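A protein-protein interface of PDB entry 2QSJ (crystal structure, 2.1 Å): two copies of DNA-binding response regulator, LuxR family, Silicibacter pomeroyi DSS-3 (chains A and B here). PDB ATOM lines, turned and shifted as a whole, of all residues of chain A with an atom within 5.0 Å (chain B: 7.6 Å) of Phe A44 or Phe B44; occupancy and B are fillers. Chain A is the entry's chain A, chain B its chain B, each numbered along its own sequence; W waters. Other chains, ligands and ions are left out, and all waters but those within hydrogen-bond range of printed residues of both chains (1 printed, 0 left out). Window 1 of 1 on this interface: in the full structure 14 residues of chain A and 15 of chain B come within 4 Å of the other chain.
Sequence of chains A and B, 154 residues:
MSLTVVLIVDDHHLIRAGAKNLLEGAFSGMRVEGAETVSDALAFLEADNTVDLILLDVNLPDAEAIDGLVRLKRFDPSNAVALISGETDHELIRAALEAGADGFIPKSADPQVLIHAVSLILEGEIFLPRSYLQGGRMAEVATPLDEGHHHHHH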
ATOM      1  N   LEU A   7     -11.587  -8.025 -12.901  1.00  0.00           N
ATOM      2  CA  LEU A   7     -10.999  -6.866 -12.247  1.00  0.00           C
ATOM      3  C   LEU A   7     -10.446  -5.935 -13.308  1.00  0.00           C
ATOM      4  O   LEU A   7      -9.565  -6.328 -14.091  1.00  0.00           O
ATOM      5  CB  LEU A   7      -9.879  -7.291 -11.252  1.00  0.00           C
ATOM      6  CG  LEU A   7      -8.996  -6.189 -10.618  1.00  0.00           C
ATOM      7  CD1 LEU A   7      -9.825  -5.264  -9.687  1.00  0.00           C
ATOM      8  CD2 LEU A   7      -7.801  -6.844  -9.829  1.00  0.00           C
ATOM      9  N   GLU A  33     -15.163  -5.498 -10.767  1.00  0.00           N
ATOM     10  CA  GLU A  33     -14.539  -4.714  -9.708  1.00  0.00           C
ATOM     11  C   GLU A  33     -13.368  -3.925 -10.240  1.00  0.00           C
ATOM     12  O   GLU A  33     -12.863  -4.226 -11.317  1.00  0.00           O
ATOM     13  CB  GLU A  33     -14.136  -5.619  -8.544  1.00  0.00           C
ATOM     14  CG  GLU A  33     -15.384  -6.407  -8.128  1.00  0.00           C
ATOM     15  CD  GLU A  33     -15.150  -7.607  -7.220  1.00  0.00           C
ATOM     16  OE1 GLU A  33     -14.138  -8.356  -7.394  1.00  0.00           O
ATOM     17  OE2 GLU A  33     -16.063  -7.805  -6.365  1.00  0.00           O
ATOM     18  N   GLY A  34     -13.006  -2.845  -9.532  1.00  0.00           N
ATOM     19  CA  GLY A  34     -12.035  -1.890 -10.054  1.00  0.00           C
ATOM     20  C   GLY A  34     -10.824  -1.724  -9.149  1.00  0.00           C
ATOM     21  O   GLY A  34     -10.907  -1.880  -7.920  1.00  0.00           O
ATOM     22  N   ASP A  40      -2.448  -1.484  -6.110  1.00  0.00           N
ATOM     23  CA  ASP A  40      -3.811  -1.718  -5.530  1.00  0.00           C
ATOM     24  C   ASP A  40      -4.402  -3.023  -6.002  1.00  0.00           C
ATOM     25  O   ASP A  40      -5.019  -3.755  -5.239  1.00  0.00           O
ATOM     26  CB  ASP A  40      -4.706  -0.566  -5.931  1.00  0.00           C
ATOM     27  CG  ASP A  40      -4.419   0.680  -5.086  1.00  0.00           C
ATOM     28  OD1 ASP A  40      -3.933   0.501  -3.947  1.00  0.00           O
ATOM     29  OD2 ASP A  40      -4.701   1.786  -5.549  1.00  0.00           O
ATOM     30  N   ALA A  41      -4.179  -3.358  -7.274  1.00  0.00           N
ATOM     31  CA  ALA A  41      -4.667  -4.672  -7.771  1.00  0.00           C
ATOM     32  C   ALA A  41      -4.005  -5.813  -7.014  1.00  0.00           C
ATOM     33  O   ALA A  41      -4.646  -6.777  -6.607  1.00  0.00           O
ATOM     34  CB  ALA A  41      -4.418  -4.778  -9.285  1.00  0.00           C
ATOM     35  N   LEU A  42      -2.695  -5.715  -6.791  1.00  0.00           N
ATOM     36  CA  LEU A  42      -1.988  -6.799  -6.086  1.00  0.00           C
ATOM     37  C   LEU A  42      -2.436  -6.935  -4.655  1.00  0.00           C
ATOM     38  O   LEU A  42      -2.607  -8.035  -4.169  1.00  0.00           O
ATOM     39  CB  LEU A  42      -0.457  -6.570  -6.137  1.00  0.00           C
ATOM     40  CG  LEU A  42       0.221  -6.780  -7.505  1.00  0.00           C
ATOM     41  CD1 LEU A  42       1.618  -6.109  -7.503  1.00  0.00           C
ATOM     42  CD2 LEU A  42       0.354  -8.270  -7.735  1.00  0.00           C
ATOM     43  N   ALA A  43      -2.667  -5.824  -3.960  1.00  0.00           N
ATOM     44  CA  ALA A  43      -3.220  -5.875  -2.581  1.00  0.00           C
ATOM     45  C   ALA A  43      -4.603  -6.503  -2.566  1.00  0.00           C
ATOM     46  O   ALA A  43      -4.973  -7.232  -1.628  1.00  0.00           O
ATOM     47  CB  ALA A  43      -3.342  -4.410  -2.071  1.00  0.00           C
ATOM     48  N   PHE A  44      -5.426  -6.161  -3.579  1.00  0.00           N
ATOM     49  CA  PHE A  44      -6.757  -6.778  -3.708  1.00  0.00           C
ATOM     50  C   PHE A  44      -6.622  -8.312  -3.824  1.00  0.00           C
ATOM     51  O   PHE A  44      -7.297  -9.114  -3.125  1.00  0.00           O
ATOM     52  CB  PHE A  44      -7.456  -6.167  -4.962  1.00  0.00           C
ATOM     53  CG  PHE A  44      -8.824  -6.783  -5.280  1.00  0.00           C
ATOM     54  CD1 PHE A  44      -9.942  -6.438  -4.523  1.00  0.00           C
ATOM     55  CD2 PHE A  44      -8.966  -7.718  -6.304  1.00  0.00           C
ATOM     56  CE1 PHE A  44     -11.216  -7.007  -4.791  1.00  0.00           C
ATOM     57  CE2 PHE A  44     -10.183  -8.271  -6.592  1.00  0.00           C
ATOM     58  CZ  PHE A  44     -11.329  -7.870  -5.824  1.00  0.00           C
ATOM     59  N   LEU A  45      -5.719  -8.718  -4.697  1.00  0.00           N
ATOM     60  CA  LEU A  45      -5.456 -10.140  -4.914  1.00  0.00           C
ATOM     61  C   LEU A  45      -4.878 -10.872  -3.698  1.00  0.00           C
ATOM     62  O   LEU A  45      -5.231 -11.992  -3.463  1.00  0.00           O
ATOM     63  CB  LEU A  45      -4.522 -10.334  -6.155  1.00  0.00           C
ATOM     64  CG  LEU A  45      -5.191  -9.997  -7.502  1.00  0.00           C
ATOM     65  CD1 LEU A  45      -4.137  -9.972  -8.585  1.00  0.00           C
ATOM     66  CD2 LEU A  45      -6.386 -10.844  -7.858  1.00  0.00           C
ATOM     67  N   GLU A  46      -4.009 -10.245  -2.919  1.00  0.00           N
ATOM     68  CA  GLU A  46      -3.537 -10.923  -1.664  1.00  0.00           C
ATOM     69  C   GLU A  46      -4.630 -11.241  -0.681  1.00  0.00           C
ATOM     70  O   GLU A  46      -4.608 -12.297  -0.043  1.00  0.00           O
ATOM     71  CB  GLU A  46      -2.562 -10.077  -0.924  1.00  0.00           C
ATOM     72  CG  GLU A  46      -1.741  -9.249  -1.802  1.00  0.00           C
ATOM     73  CD  GLU A  46      -0.360  -9.799  -2.024  1.00  0.00           C
ATOM     74  OE1 GLU A  46       0.030 -10.834  -1.365  1.00  0.00           O
ATOM     75  OE2 GLU A  46       0.337  -9.156  -2.851  1.00  0.00           O
ATOM     76  N   ALA A  47      -5.609 -10.356  -0.568  1.00  0.00           N
ATOM     77  CA  ALA A  47      -6.584 -10.443   0.478  1.00  0.00           C
ATOM     78  C   ALA A  47      -7.612 -11.504   0.101  1.00  0.00           C
ATOM     79  O   ALA A  47      -8.729 -11.531   0.617  1.00  0.00           O
ATOM     80  CB  ALA A  47      -7.228  -9.085   0.692  1.00  0.00           C
ATOM     81  N   ASP A  48      -7.189 -12.388  -0.803  1.00  0.00           N
ATOM     82  CA  ASP A  48      -7.917 -13.610  -1.162  1.00  0.00           C
ATOM     83  C   ASP A  48      -9.060 -13.361  -2.140  1.00  0.00           C
ATOM     84  O   ASP A  48      -9.899 -14.218  -2.319  1.00  0.00           O
ATOM     85  CB  ASP A  48      -8.443 -14.380   0.090  1.00  0.00           C
ATOM     86  CG  ASP A  48      -7.314 -14.666   1.145  1.00  0.00           C
ATOM     87  OD1 ASP A  48      -6.136 -14.795   0.687  1.00  0.00           O
ATOM     88  OD2 ASP A  48      -7.629 -14.720   2.403  1.00  0.00           O
ATOM     89  N   ASN A  49      -9.115 -12.183  -2.748  1.00  0.00           N
ATOM     90  CA  ASN A  49     -10.208 -11.891  -3.673  1.00  0.00           C
ATOM     91  C   ASN A  49      -9.912 -12.582  -5.002  1.00  0.00           C
ATOM     92  O   ASN A  49      -8.883 -12.317  -5.607  1.00  0.00           O
ATOM     93  CB  ASN A  49     -10.329 -10.403  -3.845  1.00  0.00           C
ATOM     94  CG  ASN A  49     -10.726  -9.723  -2.562  1.00  0.00           C
ATOM     95  OD1 ASN A  49     -11.803  -9.968  -2.042  1.00  0.00           O
ATOM     96  ND2 ASN A  49      -9.859  -8.859  -2.059  1.00  0.00           N
ATOM     97  N   VAL A  51     -10.478 -13.778  -9.026  1.00  0.00           N
ATOM     98  CA  VAL A  51     -10.985 -13.237 -10.289  1.00  0.00           C
ATOM     99  C   VAL A  51     -10.810 -14.247 -11.435  1.00  0.00           C
ATOM    100  O   VAL A  51      -9.910 -15.119 -11.396  1.00  0.00           O
ATOM    101  CB  VAL A  51     -10.237 -11.902 -10.676  1.00  0.00           C
ATOM    102  CG1 VAL A  51     -10.399 -10.844  -9.566  1.00  0.00           C
ATOM    103  CG2 VAL A  51      -8.777 -12.170 -10.900  1.00  0.00           C
ATOM    104  N   VAL B   5     -22.730  -7.180   0.134  1.00  0.00           N
ATOM    105  CA  VAL B   5     -21.285  -7.257   0.123  1.00  0.00           C
ATOM    106  C   VAL B   5     -20.714  -6.923   1.488  1.00  0.00           C
ATOM    107  O   VAL B   5     -20.967  -5.843   2.022  1.00  0.00           O
ATOM    108  CB  VAL B   5     -20.618  -6.310  -0.940  1.00  0.00           C
ATOM    109  CG1 VAL B   5     -19.108  -6.431  -0.833  1.00  0.00           C
ATOM    110  CG2 VAL B   5     -21.050  -6.682  -2.299  1.00  0.00           C
ATOM    111  N   VAL B   6     -19.925  -7.847   2.039  1.00  0.00           N
ATOM    112  CA  VAL B   6     -19.262  -7.604   3.319  1.00  0.00           C
ATOM    113  C   VAL B   6     -17.767  -7.562   3.021  1.00  0.00           C
ATOM    114  O   VAL B   6     -17.266  -8.476   2.371  1.00  0.00           O
ATOM    115  CB  VAL B   6     -19.563  -8.760   4.329  1.00  0.00           C
ATOM    116  CG1 VAL B   6     -18.824  -8.528   5.634  1.00  0.00           C
ATOM    117  CG2 VAL B   6     -21.067  -8.883   4.571  1.00  0.00           C
ATOM    118  N   LEU B   7     -17.081  -6.492   3.436  1.00  0.00           N
ATOM    119  CA  LEU B   7     -15.665  -6.406   3.336  1.00  0.00           C
ATOM    120  C   LEU B   7     -14.983  -6.738   4.690  1.00  0.00           C
ATOM    121  O   LEU B   7     -15.215  -6.076   5.698  1.00  0.00           O
ATOM    122  CB  LEU B   7     -15.242  -4.992   2.868  1.00  0.00           C
ATOM    123  CG  LEU B   7     -13.745  -4.724   2.664  1.00  0.00           C
ATOM    124  CD1 LEU B   7     -13.321  -5.587   1.460  1.00  0.00           C
ATOM    125  CD2 LEU B   7     -13.461  -3.226   2.353  1.00  0.00           C
ATOM    126  N   ARG B  16      -9.626 -14.048   7.468  1.00  0.00           N
ATOM    127  CA  ARG B  16     -10.474 -13.743   6.281  1.00  0.00           C
ATOM    128  C   ARG B  16     -11.235 -14.934   5.712  1.00  0.00           C
ATOM    129  O   ARG B  16     -12.432 -14.837   5.443  1.00  0.00           O
ATOM    130  CB  ARG B  16      -9.666 -13.137   5.103  1.00  0.00           C
ATOM    131  CG  ARG B  16      -9.091 -11.691   5.328  1.00  0.00           C
ATOM    132  CD  ARG B  16      -8.424 -11.071   4.037  1.00  0.00           C
ATOM    133  NE  ARG B  16      -7.355 -11.929   3.482  1.00  0.00           N
ATOM    134  CZ  ARG B  16      -6.059 -11.842   3.796  1.00  0.00           C
ATOM    135  NH1 ARG B  16      -5.598 -10.913   4.650  1.00  0.00           N
ATOM    136  NH2 ARG B  16      -5.193 -12.656   3.228  1.00  0.00           N
ATOM    137  N   ARG B  31     -21.718 -11.891  -0.639  1.00  0.00           N
ATOM    138  CA  ARG B  31     -20.371 -12.059  -1.143  1.00  0.00           C
ATOM    139  C   ARG B  31     -19.457 -11.393  -0.117  1.00  0.00           C
ATOM    140  O   ARG B  31     -19.706 -10.232   0.286  1.00  0.00           O
ATOM    141  CB  ARG B  31     -20.255 -11.332  -2.466  1.00  0.00           C
ATOM    142  CG  ARG B  31     -18.810 -11.134  -2.949  1.00  0.00           C
ATOM    143  CD  ARG B  31     -18.811 -10.504  -4.334  1.00  0.00           C
ATOM    144  NE  ARG B  31     -17.461 -10.546  -4.878  1.00  0.00           N
ATOM    145  CZ  ARG B  31     -16.936 -11.608  -5.471  1.00  0.00           C
ATOM    146  NH1 ARG B  31     -17.633 -12.736  -5.601  1.00  0.00           N
ATOM    147  NH2 ARG B  31     -15.703 -11.543  -5.936  1.00  0.00           N
ATOM    148  N   GLU B  33     -15.705 -10.044   0.637  1.00  0.00           N
ATOM    149  CA  GLU B  33     -14.469  -9.653   0.006  1.00  0.00           C
ATOM    150  C   GLU B  33     -13.474  -9.293   1.096  1.00  0.00           C
ATOM    151  O   GLU B  33     -13.865  -9.025   2.224  1.00  0.00           O
ATOM    152  CB  GLU B  33     -14.705  -8.475  -0.965  1.00  0.00           C
ATOM    153  CG  GLU B  33     -15.811  -8.776  -2.017  1.00  0.00           C
ATOM    154  CD  GLU B  33     -16.209  -7.589  -2.915  1.00  0.00           C
ATOM    155  OE1 GLU B  33     -16.021  -6.411  -2.536  1.00  0.00           O
ATOM    156  OE2 GLU B  33     -16.833  -7.838  -3.966  1.00  0.00           O
ATOM    157  N   GLY B  34     -12.196  -9.272   0.757  1.00  0.00           N
ATOM    158  CA  GLY B  34     -11.150  -9.007   1.761  1.00  0.00           C
ATOM    159  C   GLY B  34     -10.339  -7.783   1.425  1.00  0.00           C
ATOM    160  O   GLY B  34     -10.205  -7.407   0.263  1.00  0.00           O
ATOM    161  N   ALA B  35      -9.754  -7.189   2.457  1.00  0.00           N
ATOM    162  CA  ALA B  35      -8.710  -6.169   2.303  1.00  0.00           C
ATOM    163  C   ALA B  35      -7.687  -6.435   3.413  1.00  0.00           C
ATOM    164  O   ALA B  35      -8.050  -6.754   4.557  1.00  0.00           O
ATOM    165  CB  ALA B  35      -9.289  -4.750   2.459  1.00  0.00           C
ATOM    166  N   GLU B  36      -6.409  -6.285   3.075  1.00  0.00           N
ATOM    167  CA  GLU B  36      -5.347  -6.523   4.030  1.00  0.00           C
ATOM    168  C   GLU B  36      -5.330  -5.502   5.145  1.00  0.00           C
ATOM    169  O   GLU B  36      -5.133  -5.919   6.251  1.00  0.00           O
ATOM    170  CB  GLU B  36      -3.956  -6.584   3.357  1.00  0.00           C
ATOM    171  CG  GLU B  36      -3.804  -7.772   2.357  1.00  0.00           C
ATOM    172  CD  GLU B  36      -2.370  -7.861   1.917  1.00  0.00           C
ATOM    173  OE1 GLU B  36      -1.973  -7.044   1.030  1.00  0.00           O
ATOM    174  OE2 GLU B  36      -1.623  -8.691   2.493  1.00  0.00           O
ATOM    175  N   VAL B  38      -6.615  -1.184   6.587  1.00  0.00           N
ATOM    176  CA  VAL B  38      -7.546  -0.037   6.415  1.00  0.00           C
ATOM    177  C   VAL B  38      -7.147   0.804   5.220  1.00  0.00           C
ATOM    178  O   VAL B  38      -7.992   1.248   4.472  1.00  0.00           O
ATOM    179  CB  VAL B  38      -7.676   0.843   7.702  1.00  0.00           C
ATOM    180  CG1 VAL B  38      -8.592   2.075   7.482  1.00  0.00           C
ATOM    181  CG2 VAL B  38      -8.218  -0.009   8.823  1.00  0.00           C
ATOM    182  N   SER B  39      -5.846   1.011   5.029  1.00  0.00           N
ATOM    183  CA  SER B  39      -5.368   1.705   3.839  1.00  0.00           C
ATOM    184  C   SER B  39      -5.862   1.108   2.518  1.00  0.00           C
ATOM    185  O   SER B  39      -6.326   1.828   1.667  1.00  0.00           O
ATOM    186  CB  SER B  39      -3.818   1.760   3.795  1.00  0.00           C
ATOM    187  OG  SER B  39      -3.369   2.803   4.681  1.00  0.00           O
ATOM    188  N   ASP B  40      -5.724  -0.198   2.376  1.00  0.00           N
ATOM    189  CA  ASP B  40      -6.131  -0.917   1.187  1.00  0.00           C
ATOM    190  C   ASP B  40      -7.630  -0.875   1.087  1.00  0.00           C
ATOM    191  O   ASP B  40      -8.166  -0.703   0.015  1.00  0.00           O
ATOM    192  CB  ASP B  40      -5.662  -2.379   1.320  1.00  0.00           C
ATOM    193  CG  ASP B  40      -4.133  -2.508   1.212  1.00  0.00           C
ATOM    194  OD1 ASP B  40      -3.516  -1.778   0.407  1.00  0.00           O
ATOM    195  OD2 ASP B  40      -3.539  -3.339   1.924  1.00  0.00           O
ATOM    196  N   ALA B  41      -8.325  -1.005   2.219  1.00  0.00           N
ATOM    197  CA  ALA B  41      -9.787  -0.871   2.206  1.00  0.00           C
ATOM    198  C   ALA B  41     -10.210   0.509   1.714  1.00  0.00           C
ATOM    199  O   ALA B  41     -11.137   0.628   0.934  1.00  0.00           O
ATOM    200  CB  ALA B  41     -10.355  -1.160   3.611  1.00  0.00           C
ATOM    201  N   LEU B  42      -9.501   1.579   2.114  1.00  0.00           N
ATOM    202  CA  LEU B  42      -9.889   2.931   1.666  1.00  0.00           C
ATOM    203  C   LEU B  42      -9.602   3.148   0.193  1.00  0.00           C
ATOM    204  O   LEU B  42     -10.408   3.783  -0.497  1.00  0.00           O
ATOM    205  CB  LEU B  42      -9.207   4.044   2.472  1.00  0.00           C
ATOM    206  CG  LEU B  42      -9.769   4.182   3.898  1.00  0.00           C
ATOM    207  CD1 LEU B  42      -8.745   4.838   4.759  1.00  0.00           C
ATOM    208  CD2 LEU B  42     -11.072   4.969   3.820  1.00  0.00           C
ATOM    209  N   ALA B  43      -8.479   2.622  -0.302  1.00  0.00           N
ATOM    210  CA  ALA B  43      -8.237   2.638  -1.769  1.00  0.00           C
ATOM    211  C   ALA B  43      -9.344   1.925  -2.571  1.00  0.00           C
ATOM    212  O   ALA B  43      -9.821   2.408  -3.631  1.00  0.00           O
ATOM    213  CB  ALA B  43      -6.850   2.082  -2.058  1.00  0.00           C
ATOM    214  N   PHE B  44      -9.797   0.759  -2.074  1.00  0.00           N
ATOM    215  CA  PHE B  44     -10.783  -0.065  -2.798  1.00  0.00           C
ATOM    216  C   PHE B  44     -12.094   0.723  -2.864  1.00  0.00           C
ATOM    217  O   PHE B  44     -12.772   0.808  -3.902  1.00  0.00           O
ATOM    218  CB  PHE B  44     -10.964  -1.372  -1.989  1.00  0.00           C
ATOM    219  CG  PHE B  44     -12.015  -2.349  -2.532  1.00  0.00           C
ATOM    220  CD1 PHE B  44     -11.807  -3.041  -3.727  1.00  0.00           C
ATOM    221  CD2 PHE B  44     -13.134  -2.658  -1.784  1.00  0.00           C
ATOM    222  CE1 PHE B  44     -12.747  -3.912  -4.205  1.00  0.00           C
ATOM    223  CE2 PHE B  44     -14.064  -3.552  -2.241  1.00  0.00           C
ATOM    224  CZ  PHE B  44     -13.853  -4.225  -3.454  1.00  0.00           C
ATOM    225  N   LEU B  45     -12.442   1.318  -1.747  1.00  0.00           N
ATOM    226  CA  LEU B  45     -13.658   2.131  -1.665  1.00  0.00           C
ATOM    227  C   LEU B  45     -13.588   3.432  -2.506  1.00  0.00           C
ATOM    228  O   LEU B  45     -14.580   3.814  -3.161  1.00  0.00           O
ATOM    229  CB  LEU B  45     -13.968   2.494  -0.194  1.00  0.00           C
ATOM    230  CG  LEU B  45     -14.303   1.388   0.812  1.00  0.00           C
ATOM    231  CD1 LEU B  45     -14.586   2.079   2.232  1.00  0.00           C
ATOM    232  CD2 LEU B  45     -15.471   0.547   0.393  1.00  0.00           C
ATOM    233  N   GLU B  46     -12.447   4.121  -2.465  1.00  0.00           N
ATOM    234  CA  GLU B  46     -12.282   5.351  -3.301  1.00  0.00           C
ATOM    235  C   GLU B  46     -12.402   5.054  -4.775  1.00  0.00           C
ATOM    236  O   GLU B  46     -12.812   5.940  -5.527  1.00  0.00           O
ATOM    237  CB  GLU B  46     -10.936   6.002  -3.178  1.00  0.00           C
ATOM    238  CG  GLU B  46     -10.506   6.418  -1.808  1.00  0.00           C
ATOM    239  CD  GLU B  46      -9.084   6.888  -1.831  1.00  0.00           C
ATOM    240  OE1 GLU B  46      -8.535   7.127  -2.962  1.00  0.00           O
ATOM    241  OE2 GLU B  46      -8.517   6.986  -0.712  1.00  0.00           O
ATOM    242  N   ALA B  47     -12.035   3.835  -5.182  1.00  0.00           N
ATOM    243  CA  ALA B  47     -12.104   3.435  -6.578  1.00  0.00           C
ATOM    244  C   ALA B  47     -13.537   3.292  -7.003  1.00  0.00           C
ATOM    245  O   ALA B  47     -13.797   3.045  -8.210  1.00  0.00           O
ATOM    246  CB  ALA B  47     -11.328   2.075  -6.828  1.00  0.00           C
ATOM    247  N   ASP B  48     -14.464   3.435  -6.058  1.00  0.00           N
ATOM    248  CA  ASP B  48     -15.944   3.339  -6.336  1.00  0.00           C
ATOM    249  C   ASP B  48     -16.449   1.909  -6.371  1.00  0.00           C
ATOM    250  O   ASP B  48     -17.474   1.595  -7.028  1.00  0.00           O
ATOM    251  CB  ASP B  48     -16.392   4.181  -7.582  1.00  0.00           C
ATOM    252  CG  ASP B  48     -17.941   4.348  -7.667  1.00  0.00           C
ATOM    253  OD1 ASP B  48     -18.564   4.385  -6.573  1.00  0.00           O
ATOM    254  OD2 ASP B  48     -18.542   4.390  -8.813  1.00  0.00           O
ATOM    255  N   ASN B  49     -15.728   1.020  -5.660  1.00  0.00           N
ATOM    256  CA  ASN B  49     -16.252  -0.336  -5.346  1.00  0.00           C
ATOM    257  C   ASN B  49     -17.168  -0.232  -4.133  1.00  0.00           C
ATOM    258  O   ASN B  49     -16.855   0.430  -3.180  1.00  0.00           O
ATOM    259  CB  ASN B  49     -15.098  -1.301  -5.045  1.00  0.00           C
ATOM    260  CG  ASN B  49     -14.216  -1.543  -6.230  1.00  0.00           C
ATOM    261  OD1 ASN B  49     -14.615  -2.239  -7.151  1.00  0.00           O
ATOM    262  ND2 ASN B  49     -12.977  -1.025  -6.192  1.00  0.00           N
ATOM    263  N   THR B  50     -18.323  -0.859  -4.172  1.00  0.00           N
ATOM    264  CA  THR B  50     -19.285  -0.616  -3.113  1.00  0.00           C
ATOM    265  C   THR B  50     -19.434  -1.851  -2.254  1.00  0.00           C
ATOM    266  O   THR B  50     -19.183  -2.963  -2.709  1.00  0.00           O
ATOM    267  CB  THR B  50     -20.666  -0.199  -3.688  1.00  0.00           C
ATOM    268  OG1 THR B  50     -21.103  -1.231  -4.569  1.00  0.00           O
ATOM    269  CG2 THR B  50     -20.538   1.142  -4.447  1.00  0.00           C
ATOM    270  N   VAL B  51     -19.794  -1.614  -0.996  1.00  0.00           N
ATOM    271  CA  VAL B  51     -20.009  -2.644  -0.018  1.00  0.00           C
ATOM    272  C   VAL B  51     -21.191  -2.274   0.852  1.00  0.00           C
ATOM    273  O   VAL B  51     -21.623  -1.118   0.879  1.00  0.00           O
ATOM    274  CB  VAL B  51     -18.765  -2.826   0.925  1.00  0.00           C
ATOM    275  CG1 VAL B  51     -17.464  -3.004   0.123  1.00  0.00           C
ATOM    276  CG2 VAL B  51     -18.623  -1.662   1.910  1.00  0.00           C
ATOM    277  N   PHE B  75     -14.856   8.693   5.665  1.00  0.00           N
ATOM    278  CA  PHE B  75     -14.867   8.414   4.237  1.00  0.00           C
ATOM    279  C   PHE B  75     -16.230   8.061   3.618  1.00  0.00           C
ATOM    280  O   PHE B  75     -16.588   8.628   2.613  1.00  0.00           O
ATOM    281  CB  PHE B  75     -13.802   7.385   3.852  1.00  0.00           C
ATOM    282  CG  PHE B  75     -13.713   7.165   2.371  1.00  0.00           C
ATOM    283  CD1 PHE B  75     -12.956   8.029   1.583  1.00  0.00           C
ATOM    284  CD2 PHE B  75     -14.442   6.148   1.766  1.00  0.00           C
ATOM    285  CE1 PHE B  75     -12.881   7.868   0.215  1.00  0.00           C
ATOM    286  CE2 PHE B  75     -14.391   5.979   0.359  1.00  0.00           C
ATOM    287  CZ  PHE B  75     -13.597   6.830  -0.403  1.00  0.00           C
HETATM  288  O   HOH W   1      -6.017  -5.570   0.285  1.00  0.00           O
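OE2 of Glu A33 lies within salt-bridge range of NE of Arg B31 (3.4 Å). OE2 of Glu A33 sits close to OE2 of Glu B33, 2.5 Å away. The side-chain amide nitrogen (ND2) of Asn B49 is in hydrogen-bond range of the backbone carbonyl oxygen (O) of Gly A34, at 2.8 Å. NH2 of Arg B16 lies within hydrogen-bond range of O of Glu A46 (3.3 Å). The guanidinium group (NE) of Arg B16 sits at hydrogen-bond distance from the backbone carbonyl oxygen (O) of Ala A47, at 3.2 Å. The side-chain carboxylate (OD2) of Asp A48 is in salt-bridge range of the guanidinium group (NE) of Arg B16 (3.0 Å). The side-chain amide nitrogen (ND2) of Asn A49 sits at hydrogen-bond distance from the backbone carbonyl oxygen (O) of Gly B34, 2.8 Å away.
The backbone carbonyl oxygen of Phe A44 lies within hydrogen-bond range of the side-chain amide nitrogen of Asn A49 (2.8 Å). The backbone NH (N) of Val B6 is in hydrogen-bond range of the backbone carbonyl oxygen (O) of Arg B31 (3.0 Å). The backbone carbonyl oxygen of Val B6 sits at hydrogen-bond distance from the backbone NH of Glu B33 (2.8 Å). The side-chain carboxylate (OE2) of Glu B33 lies within salt-bridge range of the guanidinium group (NE) of Arg B31 (2.9 Å). ND2 of Asn B49 sits at hydrogen-bond distance from O of Phe B44 (2.9 Å).
Among the printed residues, pairs that only touch across the chains: Glu A33 with Asn B49 (3.6 Å), Asp A40 with Ala B43 (3.8 Å), Ala A43 with Glu B36 (3.995 Å), Ala A43 with Asp B40 (3.6 Å), Phe A44 with Phe B44 (3.5 Å), Glu A46 with Glu B36 (3.6 Å), Ala A47 with Gly B34 (3.4 Å), Ala A47 with Ala B35 (3.6 Å), Ala A47 with Glu B36 (3.8 Å) and Asn A49 with Glu B33 (3.4 Å).
Phe A44 touches just one residue of chain B: Phe B44. Of the printed residues of chain A, Phe B44 touches Phe A44 (3.5 Å). Of the printed residues of chain A, Asp B40 touches Ala A43. Of the printed residues of chain A, Glu B33 touches Glu A33 and Asn A49. The nearest residue of chain B that does not touch Phe A44 is Gly B34 (4.8 Å).
Printed residues of chain A that touch a printed residue of chain B: Glu A33, Gly A34, Asp A40, Ala A43, Phe A44, Glu A46, Ala A47, Asp A48 and Asn A49. Hydrophobic or aromatic side chains of chain A within 4 Å of the printed part of chain B: Ala A43, Phe A44 and Ala A47. Printed residues of chain B that touch a printed residue of chain A: Arg B16, Arg B31, Glu B33, Gly B34, Ala B35, Glu B36, Asp B40, Ala B43, Phe B44 and Asn B49.
Glu A33 touches Asn B49, and with the chains exchanged Asn A49 touches Glu B33. Gly A34 touches Asn B49, and with the chains exchanged Asn A49 touches Gly B34. Phe A44 touches its own counterpart, Phe B44. Ala A47 touches Gly B34, but with the chains exchanged Gly A34 does not touch Ala B47 (4.1 Å).
Water W1 bridges the backbone carbonyl oxygen (O) of Ala A43 and the backbone NH (N) of Glu B36.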
